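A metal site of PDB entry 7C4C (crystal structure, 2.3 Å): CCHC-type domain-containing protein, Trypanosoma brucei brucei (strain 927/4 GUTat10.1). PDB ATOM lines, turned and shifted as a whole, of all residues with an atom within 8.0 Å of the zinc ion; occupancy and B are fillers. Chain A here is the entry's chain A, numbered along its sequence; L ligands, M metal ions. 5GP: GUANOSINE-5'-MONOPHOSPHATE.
Of the 19 residues printed, 4 come within 4 Å of the zinc ion.
A ring nitrogen (NE2) of His 289 sits close to an oxygen (O6) of the ligand (3.0 Å). The side-chain sulfur (SG) of Cys 294 lies close to an oxygen (O6) of the ligand (3.8 Å). N of Phe 295 sits at hydrogen-bond distance from O6 of the ligand (2.9 Å). O of Asn 293 is in hydrogen-bond range of N1 of the ligand, 2.9 Å away.
The backbone NH (N) of Lys 296 sits close to the side-chain sulfur (SG) of Cys 294, 3.4 Å away. The side-chain sulfur (SG) of Cys 294 sits close to the backbone NH (N) of Lys 297 (3.5 Å). The side-chain sulfur of Cys 281 lies close to the backbone NH of Phe 283 (3.4 Å). N of Cys 281 is in hydrogen-bond range of O of Glu 286, 2.9 Å away. The side-chain sulfur (SG) of Cys 284 lies close to the backbone NH (N) of Glu 286, at 3.6 Å.
The zinc ion is bound by NE2 of His 289 (2.2 Å), SG of Cys 294 (2.2 Å), SG of Cys 281 (2.2 Å) and SG of Cys 284 (2.3 Å).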
ATOM      1  N   LYS A 280      14.212 -25.855  18.201  1.00  0.00           N
ATOM      2  CA  LYS A 280      15.468 -26.557  18.485  1.00  0.00           C
ATOM      3  C   LYS A 280      16.257 -25.797  19.538  1.00  0.00           C
ATOM      4  O   LYS A 280      16.445 -24.579  19.425  1.00  0.00           O
ATOM      5  CB  LYS A 280      16.301 -26.701  17.195  1.00  0.00           C
ATOM      6  CG  LYS A 280      17.417 -27.727  17.243  1.00  0.00           C
ATOM      7  CD  LYS A 280      18.066 -27.837  15.868  1.00  0.00           C
ATOM      8  CE  LYS A 280      19.545 -27.504  15.905  1.00  0.00           C
ATOM      9  NZ  LYS A 280      20.359 -28.696  16.273  1.00  0.00           N
ATOM     10  N   CYS A 281      16.751 -26.528  20.537  1.00  0.00           N
ATOM     11  CA  CYS A 281      17.355 -25.936  21.738  1.00  0.00           C
ATOM     12  C   CYS A 281      18.794 -25.490  21.481  1.00  0.00           C
ATOM     13  O   CYS A 281      19.661 -26.319  21.184  1.00  0.00           O
ATOM     14  CB  CYS A 281      17.326 -26.928  22.881  1.00  0.00           C
ATOM     15  SG  CYS A 281      18.035 -26.227  24.344  1.00  0.00           S
ATOM     16  N   SER A 282      19.058 -24.193  21.641  1.00  0.00           N
ATOM     17  CA  SER A 282      20.405 -23.662  21.425  1.00  0.00           C
ATOM     18  C   SER A 282      21.411 -24.098  22.481  1.00  0.00           C
ATOM     19  O   SER A 282      22.613 -23.826  22.318  1.00  0.00           O
ATOM     20  CB  SER A 282      20.354 -22.127  21.373  1.00  0.00           C
ATOM     21  OG  SER A 282      20.196 -21.574  22.666  1.00  0.00           O
ATOM     22  N   PHE A 283      20.985 -24.770  23.551  1.00  0.00           N
ATOM     23  CA  PHE A 283      21.871 -25.129  24.654  1.00  0.00           C
ATOM     24  C   PHE A 283      22.197 -26.607  24.714  1.00  0.00           C
ATOM     25  O   PHE A 283      23.344 -26.965  24.989  1.00  0.00           O
ATOM     26  CB  PHE A 283      21.250 -24.700  25.995  1.00  0.00           C
ATOM     27  CG  PHE A 283      22.174 -24.910  27.174  1.00  0.00           C
ATOM     28  CD1 PHE A 283      23.152 -23.975  27.495  1.00  0.00           C
ATOM     29  CD2 PHE A 283      22.054 -26.040  27.981  1.00  0.00           C
ATOM     30  CE1 PHE A 283      24.003 -24.161  28.587  1.00  0.00           C
ATOM     31  CE2 PHE A 283      22.892 -26.231  29.071  1.00  0.00           C
ATOM     32  CZ  PHE A 283      23.879 -25.292  29.372  1.00  0.00           C
ATOM     33  N   CYS A 284      21.231 -27.490  24.489  1.00  0.00           N
ATOM     34  CA  CYS A 284      21.475 -28.926  24.476  1.00  0.00           C
ATOM     35  C   CYS A 284      21.333 -29.537  23.083  1.00  0.00           C
ATOM     36  O   CYS A 284      21.556 -30.735  22.940  1.00  0.00           O
ATOM     37  CB  CYS A 284      20.543 -29.643  25.457  1.00  0.00           C
ATOM     38  SG  CYS A 284      18.820 -29.693  24.906  1.00  0.00           S
ATOM     39  N   GLY A 285      20.957 -28.752  22.077  1.00  0.00           N
ATOM     40  CA  GLY A 285      20.874 -29.252  20.723  1.00  0.00           C
ATOM     41  C   GLY A 285      19.606 -30.024  20.385  1.00  0.00           C
ATOM     42  O   GLY A 285      19.212 -30.062  19.218  1.00  0.00           O
ATOM     43  N   GLU A 286      18.976 -30.638  21.391  1.00  0.00           N
ATOM     44  CA  GLU A 286      17.760 -31.429  21.176  1.00  0.00           C
ATOM     45  C   GLU A 286      16.700 -30.590  20.479  1.00  0.00           C
ATOM     46  O   GLU A 286      16.564 -29.389  20.707  1.00  0.00           O
ATOM     47  CB  GLU A 286      17.223 -31.965  22.502  1.00  0.00           C
ATOM     48  CG  GLU A 286      18.114 -32.987  23.153  1.00  0.00           C
ATOM     49  CD  GLU A 286      17.703 -33.369  24.576  1.00  0.00           C
ATOM     50  OE1 GLU A 286      16.510 -33.167  24.946  1.00  0.00           O
ATOM     51  OE2 GLU A 286      18.568 -33.867  25.338  1.00  0.00           O
ATOM     52  N   VAL A 287      15.931 -31.233  19.613  1.00  0.00           N
ATOM     53  CA  VAL A 287      14.854 -30.579  18.896  1.00  0.00           C
ATOM     54  C   VAL A 287      13.559 -30.845  19.651  1.00  0.00           C
ATOM     55  O   VAL A 287      13.346 -31.947  20.173  1.00  0.00           O
ATOM     56  CB  VAL A 287      14.789 -31.068  17.438  1.00  0.00           C
ATOM     57  CG1 VAL A 287      14.756 -32.587  17.390  1.00  0.00           C
ATOM     58  CG2 VAL A 287      13.619 -30.461  16.700  1.00  0.00           C
ATOM     59  N   GLY A 288      12.710 -29.816  19.761  1.00  0.00           N
ATOM     60  CA  GLY A 288      11.472 -29.966  20.500  1.00  0.00           C
ATOM     61  C   GLY A 288      11.209 -28.900  21.559  1.00  0.00           C
ATOM     62  O   GLY A 288      10.066 -28.778  22.016  1.00  0.00           O
ATOM     63  N   HIS A 289      12.232 -28.146  21.949  1.00  0.00           N
ATOM     64  CA  HIS A 289      12.079 -27.108  22.957  1.00  0.00           C
ATOM     65  C   HIS A 289      13.095 -26.004  22.702  1.00  0.00           C
ATOM     66  O   HIS A 289      14.154 -26.246  22.140  1.00  0.00           O
ATOM     67  CB  HIS A 289      12.270 -27.663  24.379  1.00  0.00           C
ATOM     68  CG  HIS A 289      13.635 -28.235  24.613  1.00  0.00           C
ATOM     69  ND1 HIS A 289      13.938 -29.557  24.351  1.00  0.00           N
ATOM     70  CD2 HIS A 289      14.777 -27.684  25.095  1.00  0.00           C
ATOM     71  CE1 HIS A 289      15.207 -29.789  24.665  1.00  0.00           C
ATOM     72  NE2 HIS A 289      15.742 -28.664  25.106  1.00  0.00           N
ATOM     73  N   THR A 290      12.749 -24.778  23.096  1.00  0.00           N
ATOM     74  CA  THR A 290      13.696 -23.674  23.068  1.00  0.00           C
ATOM     75  C   THR A 290      14.550 -23.692  24.329  1.00  0.00           C
ATOM     76  O   THR A 290      14.302 -24.460  25.265  1.00  0.00           O
ATOM     77  CB  THR A 290      12.952 -22.350  22.926  1.00  0.00           C
ATOM     78  OG1 THR A 290      12.027 -22.191  24.009  1.00  0.00           O
ATOM     79  CG2 THR A 290      12.168 -22.319  21.614  1.00  0.00           C
ATOM     80  N   ALA A 291      15.571 -22.829  24.372  1.00  0.00           N
ATOM     81  CA  ALA A 291      16.470 -22.827  25.532  1.00  0.00           C
ATOM     82  C   ALA A 291      15.791 -22.293  26.779  1.00  0.00           C
ATOM     83  O   ALA A 291      16.161 -22.688  27.894  1.00  0.00           O
ATOM     84  CB  ALA A 291      17.726 -22.015  25.242  1.00  0.00           C
ATOM     85  N   ARG A 292      14.798 -21.409  26.627  1.00  0.00           N
ATOM     86  CA  ARG A 292      14.078 -20.878  27.790  1.00  0.00           C
ATOM     87  C   ARG A 292      13.416 -21.976  28.607  1.00  0.00           C
ATOM     88  O   ARG A 292      13.256 -21.826  29.824  1.00  0.00           O
ATOM     89  CB  ARG A 292      13.024 -19.850  27.343  1.00  0.00           C
ATOM     90  N   ASN A 293      13.059 -23.116  27.969  1.00  0.00           N
ATOM     91  CA  ASN A 293      12.434 -24.225  28.669  1.00  0.00           C
ATOM     92  C   ASN A 293      13.320 -25.474  28.731  1.00  0.00           C
ATOM     93  O   ASN A 293      12.813 -26.575  28.949  1.00  0.00           O
ATOM     94  CB  ASN A 293      11.089 -24.587  28.025  1.00  0.00           C
ATOM     95  CG  ASN A 293      10.255 -23.365  27.718  1.00  0.00           C
ATOM     96  OD1 ASN A 293       9.863 -22.618  28.618  1.00  0.00           O
ATOM     97  ND2 ASN A 293       9.929 -23.184  26.436  1.00  0.00           N
ATOM     98  N   CYS A 294      14.640 -25.335  28.588  1.00  0.00           N
ATOM     99  CA  CYS A 294      15.529 -26.484  28.572  1.00  0.00           C
ATOM    100  C   CYS A 294      15.851 -26.959  29.983  1.00  0.00           C
ATOM    101  O   CYS A 294      16.142 -26.156  30.873  1.00  0.00           O
ATOM    102  CB  CYS A 294      16.814 -26.132  27.824  1.00  0.00           C
ATOM    103  SG  CYS A 294      18.097 -27.411  27.862  1.00  0.00           S
ATOM    104  N   PHE A 295      15.789 -28.281  30.195  1.00  0.00           N
ATOM    105  CA  PHE A 295      16.033 -28.842  31.525  1.00  0.00           C
ATOM    106  C   PHE A 295      17.507 -28.880  31.859  1.00  0.00           C
ATOM    107  O   PHE A 295      17.873 -28.836  33.049  1.00  0.00           O
ATOM    108  CB  PHE A 295      15.465 -30.251  31.660  1.00  0.00           C
ATOM    109  CG  PHE A 295      13.993 -30.380  31.339  1.00  0.00           C
ATOM    110  CD1 PHE A 295      13.065 -29.529  31.901  1.00  0.00           C
ATOM    111  CD2 PHE A 295      13.560 -31.387  30.499  1.00  0.00           C
ATOM    112  CE1 PHE A 295      11.719 -29.660  31.611  1.00  0.00           C
ATOM    113  CE2 PHE A 295      12.225 -31.524  30.202  1.00  0.00           C
ATOM    114  CZ  PHE A 295      11.301 -30.664  30.763  1.00  0.00           C
ATOM    115  N   LYS A 296      18.375 -28.979  30.852  1.00  0.00           N
ATOM    116  CA  LYS A 296      19.808 -28.949  31.126  1.00  0.00           C
ATOM    117  C   LYS A 296      20.257 -27.542  31.515  1.00  0.00           C
ATOM    118  O   LYS A 296      20.994 -27.373  32.497  1.00  0.00           O
ATOM    119  CB  LYS A 296      20.600 -29.476  29.926  1.00  0.00           C
ATOM    120  CG  LYS A 296      20.275 -30.939  29.571  1.00  0.00           C
ATOM    121  CD  LYS A 296      21.468 -31.661  28.943  1.00  0.00           C
ATOM    122  CE  LYS A 296      21.134 -33.121  28.585  1.00  0.00           C
ATOM    123  NZ  LYS A 296      20.108 -33.239  27.509  1.00  0.00           N
ATOM    124  N   LYS A 297      19.778 -26.519  30.804  1.00  0.00           N
ATOM    125  CA  LYS A 297      20.141 -25.144  31.138  1.00  0.00           C
ATOM    126  C   LYS A 297      19.426 -24.638  32.383  1.00  0.00           C
ATOM    127  O   LYS A 297      19.994 -23.846  33.131  1.00  0.00           O
ATOM    128  CB  LYS A 297      19.854 -24.228  29.950  1.00  0.00           C
ATOM    129  CG  LYS A 297      20.360 -22.803  30.104  1.00  0.00           C
ATOM    130  CD  LYS A 297      20.254 -22.049  28.789  1.00  0.00           C
ATOM    131  CE  LYS A 297      21.347 -21.005  28.695  1.00  0.00           C
ATOM    132  NZ  LYS A 297      21.021 -19.927  27.720  1.00  0.00           N
ATOM    133  N   HIS A 298      18.195 -25.078  32.615  1.00  0.00           N
ATOM    134  CA  HIS A 298      17.435 -24.649  33.795  1.00  0.00           C
ATOM    135  C   HIS A 298      16.949 -25.891  34.521  1.00  0.00           C
ATOM    136  O   HIS A 298      15.807 -26.331  34.339  1.00  0.00           O
ATOM    137  CB  HIS A 298      16.281 -23.732  33.395  1.00  0.00           C
ATOM    138  CG  HIS A 298      16.712 -22.567  32.569  1.00  0.00           C
ATOM    139  ND1 HIS A 298      16.522 -22.509  31.203  1.00  0.00           N
ATOM    140  CD2 HIS A 298      17.390 -21.437  32.905  1.00  0.00           C
ATOM    141  CE1 HIS A 298      17.034 -21.389  30.737  1.00  0.00           C
ATOM    142  NE2 HIS A 298      17.566 -20.721  31.752  1.00  0.00           N
HETATM  143  C4' 5GP L   1      10.568 -35.928  25.803  1.00  0.00           C
HETATM  144  O4' 5GP L   1      10.875 -34.813  26.648  1.00  0.00           O
HETATM  145  C3' 5GP L   1      10.502 -35.399  24.387  1.00  0.00           C
HETATM  146  O3' 5GP L   1       9.141 -35.186  24.014  1.00  0.00           O
HETATM  147  C2' 5GP L   1      11.140 -34.034  24.419  1.00  0.00           C
HETATM  148  O2' 5GP L   1      10.398 -33.136  23.581  1.00  0.00           O
HETATM  149  C1' 5GP L   1      11.045 -33.625  25.870  1.00  0.00           C
HETATM  150  N9  5GP L   1      12.303 -32.930  26.268  1.00  0.00           N
HETATM  151  C8  5GP L   1      13.548 -33.423  26.166  1.00  0.00           C
HETATM  152  N7  5GP L   1      14.412 -32.489  26.641  1.00  0.00           N
HETATM  153  C5  5GP L   1      13.696 -31.407  27.025  1.00  0.00           C
HETATM  154  C6  5GP L   1      14.026 -30.165  27.576  1.00  0.00           C
HETATM  155  O6  5GP L   1      15.220 -29.856  27.805  1.00  0.00           O
HETATM  156  N1  5GP L   1      13.046 -29.295  27.856  1.00  0.00           N
HETATM  157  C2  5GP L   1      11.761 -29.582  27.621  1.00  0.00           C
HETATM  158  N2  5GP L   1      10.807 -28.666  27.917  1.00  0.00           N
HETATM  159  N3  5GP L   1      11.409 -30.776  27.094  1.00  0.00           N
HETATM  160  C4  5GP L   1      12.358 -31.701  26.800  1.00  0.00           C
HETATM  161 ZN    ZN M   1      17.690 -27.925  25.754  1.00  0.00          ZN
HETATM  162 MN    MN M   2      16.468 -33.336  27.018  1.00  0.00          MN
